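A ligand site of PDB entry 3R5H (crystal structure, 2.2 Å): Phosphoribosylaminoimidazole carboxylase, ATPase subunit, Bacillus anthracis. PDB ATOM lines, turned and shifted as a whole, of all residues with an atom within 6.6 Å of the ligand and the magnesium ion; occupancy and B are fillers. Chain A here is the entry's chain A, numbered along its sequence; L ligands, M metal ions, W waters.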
ATOM      1  N   ARG A 113       2.250   8.186  -8.367  1.00  0.00           N
ATOM      2  CA  ARG A 113       3.144   8.408  -7.237  1.00  0.00           C
ATOM      3  C   ARG A 113       2.558   9.388  -6.227  1.00  0.00           C
ATOM      4  O   ARG A 113       2.661   9.190  -5.016  1.00  0.00           O
ATOM      5  CB  ARG A 113       4.513   8.907  -7.703  1.00  0.00           C
ATOM      6  CG  ARG A 113       5.367   7.856  -8.423  1.00  0.00           C
ATOM      7  CD  ARG A 113       6.809   8.369  -8.512  1.00  0.00           C
ATOM      8  NE  ARG A 113       7.701   7.535  -9.322  1.00  0.00           N
ATOM      9  CZ  ARG A 113       8.517   6.612  -8.822  1.00  0.00           C
ATOM     10  NH1 ARG A 113       9.304   5.917  -9.638  1.00  0.00           N
ATOM     11  NH2 ARG A 113       8.559   6.372  -7.514  1.00  0.00           N
ATOM     12  N   LYS A 117       1.402   8.453  -2.401  1.00  0.00           N
ATOM     13  CA  LYS A 117       1.916   9.189  -1.270  1.00  0.00           C
ATOM     14  C   LYS A 117       0.827   9.810  -0.399  1.00  0.00           C
ATOM     15  O   LYS A 117       0.908   9.746   0.850  1.00  0.00           O
ATOM     16  CB  LYS A 117       2.985  10.201  -1.721  1.00  0.00           C
ATOM     17  CG  LYS A 117       4.351   9.538  -1.773  1.00  0.00           C
ATOM     18  CD  LYS A 117       5.472  10.454  -2.173  1.00  0.00           C
ATOM     19  CE  LYS A 117       6.827   9.901  -1.721  1.00  0.00           C
ATOM     20  NZ  LYS A 117       7.155   8.520  -2.241  1.00  0.00           N
ATOM     21  N   ALA A 128       8.849  10.944   2.417  1.00  0.00           N
ATOM     22  CA  ALA A 128       9.610  12.135   2.091  1.00  0.00           C
ATOM     23  C   ALA A 128       8.642  13.263   1.722  1.00  0.00           C
ATOM     24  O   ALA A 128       7.612  13.022   1.069  1.00  0.00           O
ATOM     25  CB  ALA A 128      10.575  11.868   0.944  1.00  0.00           C
ATOM     26  N   THR A 129       8.961  14.481   2.154  1.00  0.00           N
ATOM     27  CA  THR A 129       8.138  15.656   1.813  1.00  0.00           C
ATOM     28  C   THR A 129       8.120  15.773   0.292  1.00  0.00           C
ATOM     29  O   THR A 129       9.142  15.599  -0.359  1.00  0.00           O
ATOM     30  CB  THR A 129       8.681  16.945   2.508  1.00  0.00           C
ATOM     31  OG1 THR A 129       8.781  16.721   3.933  1.00  0.00           O
ATOM     32  CG2 THR A 129       7.773  18.166   2.246  1.00  0.00           C
ATOM     33  N   SER A 150      16.902  17.413  -3.771  1.00  0.00           N
ATOM     34  CA  SER A 150      15.533  16.945  -3.994  1.00  0.00           C
ATOM     35  C   SER A 150      15.527  16.096  -5.247  1.00  0.00           C
ATOM     36  O   SER A 150      16.492  16.101  -5.997  1.00  0.00           O
ATOM     37  CB  SER A 150      14.573  18.129  -4.149  1.00  0.00           C
ATOM     38  OG  SER A 150      14.979  18.971  -5.221  1.00  0.00           O
ATOM     39  N   VAL A 151      14.436  15.355  -5.446  1.00  0.00           N
ATOM     40  CA  VAL A 151      14.305  14.442  -6.584  1.00  0.00           C
ATOM     41  C   VAL A 151      12.951  14.630  -7.284  1.00  0.00           C
ATOM     42  O   VAL A 151      11.889  14.498  -6.660  1.00  0.00           O
ATOM     43  CB  VAL A 151      14.322  12.963  -6.155  1.00  0.00           C
ATOM     44  CG1 VAL A 151      14.620  12.081  -7.340  1.00  0.00           C
ATOM     45  CG2 VAL A 151      15.317  12.747  -5.044  1.00  0.00           C
ATOM     46  N   LYS A 153      10.491  13.097 -10.040  1.00  0.00           N
ATOM     47  CA  LYS A 153      10.164  11.849 -10.723  1.00  0.00           C
ATOM     48  C   LYS A 153       8.821  12.001 -11.427  1.00  0.00           C
ATOM     49  O   LYS A 153       8.006  12.813 -10.996  1.00  0.00           O
ATOM     50  CB  LYS A 153       9.999  10.688  -9.717  1.00  0.00           C
ATOM     51  CG  LYS A 153      11.038  10.566  -8.636  1.00  0.00           C
ATOM     52  CD  LYS A 153      10.564   9.481  -7.671  1.00  0.00           C
ATOM     53  CE  LYS A 153      11.537   9.310  -6.538  1.00  0.00           C
ATOM     54  NZ  LYS A 153      10.957   8.483  -5.442  1.00  0.00           N
ATOM     55  N   GLY A 157       3.907   5.484 -15.127  1.00  0.00           N
ATOM     56  CA  GLY A 157       4.687   4.797 -16.149  1.00  0.00           C
ATOM     57  C   GLY A 157       6.146   4.615 -15.796  1.00  0.00           C
ATOM     58  O   GLY A 157       6.534   4.778 -14.633  1.00  0.00           O
ATOM     59  N   GLY A 158       6.961   4.291 -16.807  1.00  0.00           N
ATOM     60  CA  GLY A 158       8.386   4.059 -16.601  1.00  0.00           C
ATOM     61  C   GLY A 158       8.588   2.723 -15.907  1.00  0.00           C
ATOM     62  O   GLY A 158       8.517   2.618 -14.682  1.00  0.00           O
ATOM     63  N   TYR A 159       8.839   1.695 -16.720  1.00  0.00           N
ATOM     64  CA  TYR A 159       9.009   0.336 -16.232  1.00  0.00           C
ATOM     65  C   TYR A 159      10.412   0.094 -15.656  1.00  0.00           C
ATOM     66  O   TYR A 159      10.717  -1.014 -15.193  1.00  0.00           O
ATOM     67  CB  TYR A 159       8.686  -0.665 -17.349  1.00  0.00           C
ATOM     68  CG  TYR A 159       7.741  -1.781 -16.932  1.00  0.00           C
ATOM     69  CD1 TYR A 159       8.050  -3.123 -17.166  1.00  0.00           C
ATOM     70  CD2 TYR A 159       6.516  -1.488 -16.303  1.00  0.00           C
ATOM     71  CE1 TYR A 159       7.177  -4.155 -16.793  1.00  0.00           C
ATOM     72  CE2 TYR A 159       5.635  -2.501 -15.921  1.00  0.00           C
ATOM     73  CZ  TYR A 159       5.967  -3.836 -16.173  1.00  0.00           C
ATOM     74  OH  TYR A 159       5.100  -4.847 -15.796  1.00  0.00           O
ATOM     75  N   ASP A 160      11.243   1.133 -15.667  1.00  0.00           N
ATOM     76  CA  ASP A 160      12.632   1.074 -15.172  1.00  0.00           C
ATOM     77  C   ASP A 160      12.983   2.156 -14.140  1.00  0.00           C
ATOM     78  O   ASP A 160      13.731   1.900 -13.184  1.00  0.00           O
ATOM     79  CB  ASP A 160      13.648   1.117 -16.330  1.00  0.00           C
ATOM     80  CG  ASP A 160      13.530   2.383 -17.188  1.00  0.00           C
ATOM     81  OD1 ASP A 160      12.568   2.505 -17.985  1.00  0.00           O
ATOM     82  OD2 ASP A 160      14.429   3.247 -17.090  1.00  0.00           O
ATOM     83  N   GLY A 161      12.455   3.358 -14.346  1.00  0.00           N
ATOM     84  CA  GLY A 161      12.817   4.537 -13.565  1.00  0.00           C
ATOM     85  C   GLY A 161      13.517   5.561 -14.432  1.00  0.00           C
ATOM     86  O   GLY A 161      14.454   6.234 -13.997  1.00  0.00           O
ATOM     87  N   LYS A 162      13.028   5.680 -15.670  1.00  0.00           N
ATOM     88  CA  LYS A 162      13.630   6.526 -16.713  1.00  0.00           C
ATOM     89  C   LYS A 162      13.455   8.016 -16.437  1.00  0.00           C
ATOM     90  O   LYS A 162      14.354   8.830 -16.710  1.00  0.00           O
ATOM     91  CB  LYS A 162      13.024   6.170 -18.079  1.00  0.00           C
ATOM     92  CG  LYS A 162      13.684   6.825 -19.303  1.00  0.00           C
ATOM     93  CD  LYS A 162      12.785   6.713 -20.541  1.00  0.00           C
ATOM     94  CE  LYS A 162      12.499   5.258 -20.904  1.00  0.00           C
ATOM     95  NZ  LYS A 162      11.193   5.105 -21.607  1.00  0.00           N
ATOM     96  N   GLN A 164      13.624  10.312 -13.924  1.00  0.00           N
ATOM     97  CA  GLN A 164      14.087  10.802 -12.641  1.00  0.00           C
ATOM     98  C   GLN A 164      15.279  11.747 -12.781  1.00  0.00           C
ATOM     99  O   GLN A 164      16.246  11.437 -13.454  1.00  0.00           O
ATOM    100  CB  GLN A 164      14.420   9.641 -11.695  1.00  0.00           C
ATOM    101  CG  GLN A 164      14.832  10.095 -10.305  1.00  0.00           C
ATOM    102  CD  GLN A 164      14.762   8.985  -9.262  1.00  0.00           C
ATOM    103  OE1 GLN A 164      13.777   8.244  -9.179  1.00  0.00           O
ATOM    104  NE2 GLN A 164      15.811   8.869  -8.450  1.00  0.00           N
ATOM    105  N   VAL A 166      17.816  14.027 -10.274  1.00  0.00           N
ATOM    106  CA  VAL A 166      18.249  14.385  -8.932  1.00  0.00           C
ATOM    107  C   VAL A 166      18.779  15.808  -8.968  1.00  0.00           C
ATOM    108  O   VAL A 166      19.650  16.140  -9.771  1.00  0.00           O
ATOM    109  CB  VAL A 166      19.316  13.408  -8.375  1.00  0.00           C
ATOM    110  CG1 VAL A 166      19.684  13.768  -6.931  1.00  0.00           C
ATOM    111  CG2 VAL A 166      18.843  11.952  -8.436  1.00  0.00           C
ATOM    112  N   GLU A 188      10.260  15.317  -4.608  1.00  0.00           N
ATOM    113  CA  GLU A 188      10.464  14.784  -3.251  1.00  0.00           C
ATOM    114  C   GLU A 188      11.741  15.353  -2.619  1.00  0.00           C
ATOM    115  O   GLU A 188      12.765  15.424  -3.293  1.00  0.00           O
ATOM    116  CB  GLU A 188      10.669  13.267  -3.280  1.00  0.00           C
ATOM    117  CG  GLU A 188       9.494  12.442  -3.754  1.00  0.00           C
ATOM    118  CD  GLU A 188       9.770  10.943  -3.625  1.00  0.00           C
ATOM    119  OE1 GLU A 188       9.020  10.140  -4.236  1.00  0.00           O
ATOM    120  OE2 GLU A 188      10.749  10.574  -2.934  1.00  0.00           O
ATOM    121  N   LYS A 189      11.688  15.702  -1.324  1.00  0.00           N
ATOM    122  CA  LYS A 189      12.924  15.899  -0.560  1.00  0.00           C
ATOM    123  C   LYS A 189      13.826  14.660  -0.701  1.00  0.00           C
ATOM    124  O   LYS A 189      13.341  13.526  -0.680  1.00  0.00           O
ATOM    125  CB  LYS A 189      12.636  16.118   0.924  1.00  0.00           C
ATOM    126  CG  LYS A 189      12.507  17.581   1.375  1.00  0.00           C
ATOM    127  CD  LYS A 189      13.014  17.746   2.817  1.00  0.00           C
ATOM    128  CE  LYS A 189      12.015  18.434   3.742  1.00  0.00           C
ATOM    129  NZ  LYS A 189      11.843  19.886   3.495  1.00  0.00           N
ATOM    130  N   TRP A 190      15.125  14.889  -0.872  1.00  0.00           N
ATOM    131  CA  TRP A 190      16.122  13.831  -0.824  1.00  0.00           C
ATOM    132  C   TRP A 190      16.244  13.314   0.611  1.00  0.00           C
ATOM    133  O   TRP A 190      16.420  14.100   1.549  1.00  0.00           O
ATOM    134  CB  TRP A 190      17.468  14.337  -1.335  1.00  0.00           C
ATOM    135  CG  TRP A 190      18.608  13.328  -1.403  1.00  0.00           C
ATOM    136  CD1 TRP A 190      19.601  13.141  -0.470  1.00  0.00           C
ATOM    137  CD2 TRP A 190      18.886  12.397  -2.463  1.00  0.00           C
ATOM    138  NE1 TRP A 190      20.462  12.147  -0.886  1.00  0.00           N
ATOM    139  CE2 TRP A 190      20.047  11.681  -2.102  1.00  0.00           C
ATOM    140  CE3 TRP A 190      18.263  12.093  -3.673  1.00  0.00           C
ATOM    141  CZ2 TRP A 190      20.601  10.674  -2.920  1.00  0.00           C
ATOM    142  CZ3 TRP A 190      18.813  11.088  -4.478  1.00  0.00           C
ATOM    143  CH2 TRP A 190      19.970  10.402  -4.095  1.00  0.00           C
ATOM    144  N   VAL A 191      16.113  11.999   0.791  1.00  0.00           N
ATOM    145  CA  VAL A 191      16.237  11.404   2.102  1.00  0.00           C
ATOM    146  C   VAL A 191      17.663  10.859   2.242  1.00  0.00           C
ATOM    147  O   VAL A 191      18.048   9.979   1.470  1.00  0.00           O
ATOM    148  CB  VAL A 191      15.220  10.232   2.295  1.00  0.00           C
ATOM    149  CG1 VAL A 191      15.234   9.753   3.738  1.00  0.00           C
ATOM    150  CG2 VAL A 191      13.811  10.660   1.901  1.00  0.00           C
ATOM    151  N   PRO A 192      18.449  11.394   3.199  1.00  0.00           N
ATOM    152  CA  PRO A 192      19.677  10.687   3.583  1.00  0.00           C
ATOM    153  C   PRO A 192      19.271   9.443   4.362  1.00  0.00           C
ATOM    154  O   PRO A 192      18.553   9.542   5.366  1.00  0.00           O
ATOM    155  CB  PRO A 192      20.402  11.691   4.532  1.00  0.00           C
ATOM    156  CG  PRO A 192      19.676  12.967   4.398  1.00  0.00           C
ATOM    157  CD  PRO A 192      18.256  12.608   3.995  1.00  0.00           C
ATOM    158  N   PHE A 193      19.652   8.278   3.846  1.00  0.00           N
ATOM    159  CA  PHE A 193      19.309   7.021   4.488  1.00  0.00           C
ATOM    160  C   PHE A 193      20.501   6.073   4.354  1.00  0.00           C
ATOM    161  O   PHE A 193      21.381   6.281   3.520  1.00  0.00           O
ATOM    162  CB  PHE A 193      18.019   6.397   3.909  1.00  0.00           C
ATOM    163  CG  PHE A 193      18.141   5.966   2.464  1.00  0.00           C
ATOM    164  CD1 PHE A 193      17.692   6.793   1.433  1.00  0.00           C
ATOM    165  CD2 PHE A 193      18.698   4.730   2.138  1.00  0.00           C
ATOM    166  CE1 PHE A 193      17.807   6.405   0.104  1.00  0.00           C
ATOM    167  CE2 PHE A 193      18.849   4.338   0.828  1.00  0.00           C
ATOM    168  CZ  PHE A 193      18.391   5.173  -0.208  1.00  0.00           C
ATOM    169  N   GLU A 196      18.029   0.671   1.909  1.00  0.00           N
ATOM    170  CA  GLU A 196      16.718   0.431   1.314  1.00  0.00           C
ATOM    171  C   GLU A 196      16.282  -0.968   1.745  1.00  0.00           C
ATOM    172  O   GLU A 196      17.035  -1.926   1.591  1.00  0.00           O
ATOM    173  CB  GLU A 196      16.774   0.485  -0.210  1.00  0.00           C
ATOM    174  CG  GLU A 196      17.133   1.833  -0.762  1.00  0.00           C
ATOM    175  CD  GLU A 196      16.657   2.033  -2.179  1.00  0.00           C
ATOM    176  OE1 GLU A 196      17.505   2.411  -3.014  1.00  0.00           O
ATOM    177  OE2 GLU A 196      15.447   1.823  -2.469  1.00  0.00           O
ATOM    178  N   HIS A 219      20.253  -1.944  -5.075  1.00  0.00           N
ATOM    179  CA  HIS A 219      19.973  -1.608  -6.477  1.00  0.00           C
ATOM    180  C   HIS A 219      21.259  -1.142  -7.189  1.00  0.00           C
ATOM    181  O   HIS A 219      22.062  -0.436  -6.618  1.00  0.00           O
ATOM    182  CB  HIS A 219      18.902  -0.513  -6.574  1.00  0.00           C
ATOM    183  CG  HIS A 219      17.567  -0.923  -6.037  1.00  0.00           C
ATOM    184  ND1 HIS A 219      17.230  -0.793  -4.696  1.00  0.00           N
ATOM    185  CD2 HIS A 219      16.485  -1.474  -6.636  1.00  0.00           C
ATOM    186  CE1 HIS A 219      16.004  -1.241  -4.510  1.00  0.00           C
ATOM    187  NE2 HIS A 219      15.534  -1.674  -5.673  1.00  0.00           N
ATOM    188  N   ASN A 222      19.457   1.336 -10.959  1.00  0.00           N
ATOM    189  CA  ASN A 222      18.010   1.335 -10.708  1.00  0.00           C
ATOM    190  C   ASN A 222      17.339  -0.007 -11.028  1.00  0.00           C
ATOM    191  O   ASN A 222      16.118  -0.076 -11.291  1.00  0.00           O
ATOM    192  CB  ASN A 222      17.304   2.467 -11.471  1.00  0.00           C
ATOM    193  CG  ASN A 222      16.048   2.955 -10.758  1.00  0.00           C
ATOM    194  OD1 ASN A 222      15.902   2.782  -9.539  1.00  0.00           O
ATOM    195  ND2 ASN A 222      15.129   3.562 -11.509  1.00  0.00           N
ATOM    196  N   GLU A 261       8.122  -0.832  -0.056  1.00  0.00           N
ATOM    197  CA  GLU A 261       9.509  -0.441  -0.164  1.00  0.00           C
ATOM    198  C   GLU A 261       9.774   0.806   0.652  1.00  0.00           C
ATOM    199  O   GLU A 261       9.011   1.773   0.591  1.00  0.00           O
ATOM    200  CB  GLU A 261       9.903  -0.227  -1.617  1.00  0.00           C
ATOM    201  CG  GLU A 261      10.045  -1.529  -2.377  1.00  0.00           C
ATOM    202  CD  GLU A 261      10.678  -1.293  -3.733  1.00  0.00           C
ATOM    203  OE1 GLU A 261       9.943  -0.931  -4.672  1.00  0.00           O
ATOM    204  OE2 GLU A 261      11.928  -1.454  -3.831  1.00  0.00           O
ATOM    205  N   PHE A 263      12.867   3.456   2.928  1.00  0.00           N
ATOM    206  CA  PHE A 263      14.218   3.952   3.200  1.00  0.00           C
ATOM    207  C   PHE A 263      14.434   3.917   4.720  1.00  0.00           C
ATOM    208  O   PHE A 263      13.578   4.369   5.474  1.00  0.00           O
ATOM    209  CB  PHE A 263      14.413   5.398   2.716  1.00  0.00           C
ATOM    210  CG  PHE A 263      14.147   5.604   1.235  1.00  0.00           C
ATOM    211  CD1 PHE A 263      13.467   6.739   0.808  1.00  0.00           C
ATOM    212  CD2 PHE A 263      14.574   4.692   0.272  1.00  0.00           C
ATOM    213  CE1 PHE A 263      13.216   6.972  -0.570  1.00  0.00           C
ATOM    214  CE2 PHE A 263      14.330   4.906  -1.093  1.00  0.00           C
ATOM    215  CZ  PHE A 263      13.649   6.054  -1.516  1.00  0.00           C
ATOM    216  N   ASN A 273       8.771   4.469   0.492  1.00  0.00           N
ATOM    217  CA  ASN A 273       9.126   4.911  -0.842  1.00  0.00           C
ATOM    218  C   ASN A 273       8.020   4.579  -1.841  1.00  0.00           C
ATOM    219  O   ASN A 273       7.492   5.458  -2.515  1.00  0.00           O
ATOM    220  CB  ASN A 273      10.450   4.273  -1.271  1.00  0.00           C
ATOM    221  CG  ASN A 273      10.828   4.566  -2.694  1.00  0.00           C
ATOM    222  OD1 ASN A 273      10.607   5.668  -3.200  1.00  0.00           O
ATOM    223  ND2 ASN A 273      11.452   3.589  -3.351  1.00  0.00           N
ATOM    224  N   GLU A 274       7.675   3.303  -1.959  1.00  0.00           N
ATOM    225  CA  GLU A 274       6.669   2.875  -2.924  1.00  0.00           C
ATOM    226  C   GLU A 274       6.029   1.529  -2.591  1.00  0.00           C
ATOM    227  O   GLU A 274       6.549   0.748  -1.783  1.00  0.00           O
ATOM    228  CB  GLU A 274       7.188   2.932  -4.384  1.00  0.00           C
ATOM    229  CG  GLU A 274       8.371   2.046  -4.662  1.00  0.00           C
ATOM    230  CD  GLU A 274       8.800   2.022  -6.114  1.00  0.00           C
ATOM    231  OE1 GLU A 274       9.924   1.485  -6.372  1.00  0.00           O
ATOM    232  OE2 GLU A 274       8.033   2.515  -7.000  1.00  0.00           O
ATOM    233  N   HIS A 280       6.623  -9.484  -5.564  1.00  0.00           N
ATOM    234  CA  HIS A 280       7.662  -8.512  -5.916  1.00  0.00           C
ATOM    235  C   HIS A 280       9.053  -9.131  -5.964  1.00  0.00           C
ATOM    236  O   HIS A 280       9.334 -10.116  -5.288  1.00  0.00           O
ATOM    237  CB  HIS A 280       7.618  -7.386  -4.881  1.00  0.00           C
ATOM    238  CG  HIS A 280       8.469  -6.205  -5.210  1.00  0.00           C
ATOM    239  ND1 HIS A 280       9.752  -6.058  -4.723  1.00  0.00           N
ATOM    240  CD2 HIS A 280       8.201  -5.088  -5.927  1.00  0.00           C
ATOM    241  CE1 HIS A 280      10.252  -4.908  -5.156  1.00  0.00           C
ATOM    242  NE2 HIS A 280       9.336  -4.304  -5.897  1.00  0.00           N
HETATM  243  P1  LIG L   1      11.699   3.358  -9.353  1.00  0.00           P
HETATM  244  O1  LIG L   1      11.605   3.812 -10.774  1.00  0.00           O
HETATM  245  O2  LIG L   1      10.418   2.732  -8.903  1.00  0.00           O
HETATM  246  O3  LIG L   1      12.930   2.557  -9.022  1.00  0.00           O
HETATM  247  P2  LIG L   1      12.288   4.962  -7.000  1.00  0.00           P
HETATM  248  O4  LIG L   1      12.462   3.611  -6.355  1.00  0.00           O
HETATM  249  O5  LIG L   1      11.302   5.943  -6.420  1.00  0.00           O
HETATM  250  O6  LIG L   1      11.870   4.762  -8.553  1.00  0.00           O
HETATM  251  O7  LIG L   1      13.706   5.704  -7.042  1.00  0.00           O
HETATM  252  C1  LIG L   1      14.849   5.023  -7.562  1.00  0.00           C
HETATM  253  C2  LIG L   1      16.015   5.161  -6.602  1.00  0.00           C
HETATM  254  O8  LIG L   1      16.336   6.548  -6.417  1.00  0.00           O
HETATM  255  C3  LIG L   1      15.689   4.616  -5.222  1.00  0.00           C
HETATM  256  O9  LIG L   1      16.074   3.247  -5.093  1.00  0.00           O
HETATM  257  C4  LIG L   1      16.505   5.491  -4.303  1.00  0.00           C
HETATM  258  O10 LIG L   1      17.838   4.959  -4.213  1.00  0.00           O
HETATM  259  C5  LIG L   1      16.604   6.810  -5.024  1.00  0.00           C
HETATM  260  N1  LIG L   1      15.603   7.751  -4.485  1.00  0.00           N
HETATM  261  C6  LIG L   1      14.359   7.962  -4.973  1.00  0.00           C
HETATM  262  N2  LIG L   1      13.689   8.899  -4.246  1.00  0.00           N
HETATM  263  C7  LIG L   1      14.526   9.312  -3.279  1.00  0.00           C
HETATM  264  C8  LIG L   1      14.466  10.282  -2.176  1.00  0.00           C
HETATM  265  N3  LIG L   1      13.365  11.035  -1.936  1.00  0.00           N
HETATM  266  N4  LIG L   1      15.579  10.387  -1.395  1.00  0.00           N
HETATM  267  C9  LIG L   1      16.691   9.664  -1.585  1.00  0.00           C
HETATM  268  N5  LIG L   1      16.797   8.772  -2.581  1.00  0.00           N
HETATM  269  C10 LIG L   1      15.773   8.554  -3.440  1.00  0.00           C
HETATM  270 MG    MG M   1      12.053   1.593  -6.672  1.00  0.00          MG
HETATM  271  O   HOH W   1      10.539  -0.890  -7.508  1.00  0.00           O
HETATM  272  O   HOH W   2      14.108  -0.426  -9.444  1.00  0.00           O
HETATM  273  O   HOH W   3      19.533   7.525  -3.107  1.00  0.00           O
HETATM  274  O   HOH W   4      13.008  -0.407  -6.960  1.00  0.00           O
HETATM  275  O   HOH W   5      13.217   1.227  -4.238  1.00  0.00           O
HETATM  276  O   HOH W   6      14.677   1.667  -7.220  1.00  0.00           O
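The side-chain carboxylate (OE1) of Glu 196 sits at hydrogen-bond distance from an oxygen (O9) of the ligand (2.7 Å).
An oxygen (O5) of the ligand is in salt-bridge range of the side-chain amino group (NZ) of Lys 153, 2.7 Å away.
N4 of the ligand lies within hydrogen-bond range of N of Val 191 (2.8 Å).
A nitrogen (N3) of the ligand is in hydrogen-bond range of the backbone carbonyl oxygen (O) of Lys 189, at 2.8 Å.
N3 of the ligand lies within hydrogen-bond range of OE2 of Glu 188, at 2.8 Å.
The guanidinium group (NH2) of Arg 113 lies within salt-bridge range of an oxygen (O5) of the ligand (3.0 Å).
An oxygen (O3) of the ligand sits close to the side-chain amide oxygen (OD1) of Asn 222 (3.0 Å).
The side-chain amide nitrogen (NE2) of Gln 164 sits at hydrogen-bond distance from an oxygen (O8) of the ligand, at 3.1 Å.
The side-chain amide oxygen of Asn 273 sits close to an oxygen (O5) of the ligand.
The side-chain carboxylate of Glu 274 is in salt-bridge range of the guanidinium group of Arg 113 (3.9 Å).
The side-chain amino group (NZ) of Lys 153 is in salt-bridge range of the side-chain carboxylate (OE1) of Glu 188, at 2.8 Å.
The backbone NH of Lys 189 is in hydrogen-bond range of the backbone carbonyl oxygen of Thr 129 (2.7 Å).
O of Glu 188 sits at hydrogen-bond distance from N of Val 151, at 2.7 Å.
NZ of Lys 117 is in salt-bridge range of OE1 of Glu 188 (3.2 Å).
ND2 of Asn 222 sits at hydrogen-bond distance from O of Asp 160.
O of Glu 261 is in hydrogen-bond range of N of Asn 273 (2.7 Å).
NZ of Lys 117 lies within hydrogen-bond range of O of Asn 273 (3.1 Å).
Val 151 touches the ligand (CG2 to C8, 3.9 Å).
Asp 160 touches the ligand (O to O1, 3.7 Å).
Gly 161 touches the ligand.
Trp 190 touches the ligand.
Phe 193 touches the ligand.
Phe 263 touches the ligand (CZ to C10, 3.8 Å).
Hydrophobic or aromatic side chains within 4 Å of the ligand: Val 151, Trp 190, Val 191, Phe 193 and Phe 263.
Within 4 Å of the ligand: Arg 113, Val 151, Lys 153, Asp 160, Gly 161, Gln 164, Glu 188, Lys 189, Trp 190, Val 191, Phe 193, Glu 196, Asn 222, Phe 263, Asn 273 and Glu 274.
The nearest printed residue that does not touch the ligand is Ala 128 (4.1 Å).
Glu 261 touches the magnesium ion.
Asn 273 touches the magnesium ion.
An oxygen (O4) of the ligand binds the magnesium ion (2.1 Å).
OE1 of Glu 274 is bound to the magnesium ion (2.2 Å).
The magnesium ion is bound by water W4, at 2.2 Å.
The magnesium ion has three donor atoms within binding distance.
Slightly farther from the magnesium ion lies water W6 (2.7 Å).
Slightly farther from the magnesium ion lies O3 of the ligand (2.7 Å).
Slightly farther from the magnesium ion lies water W5 (2.7 Å).
Water W4 bridges a ring nitrogen (NE2) of His 219 and the side-chain carboxylate (OE2) of Glu 261.
Water W6 bridges O3 of the ligand and OD1 of Asn 222.
Water W5 lies within hydrogen-bond range of OE2 of Glu 196 (2.9 Å), OE2 of Glu 261 (3.0 Å) and ND2 of Asn 273 (3.1 Å).
Water W2 bridges O of Asn 222 and O3 of the ligand.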
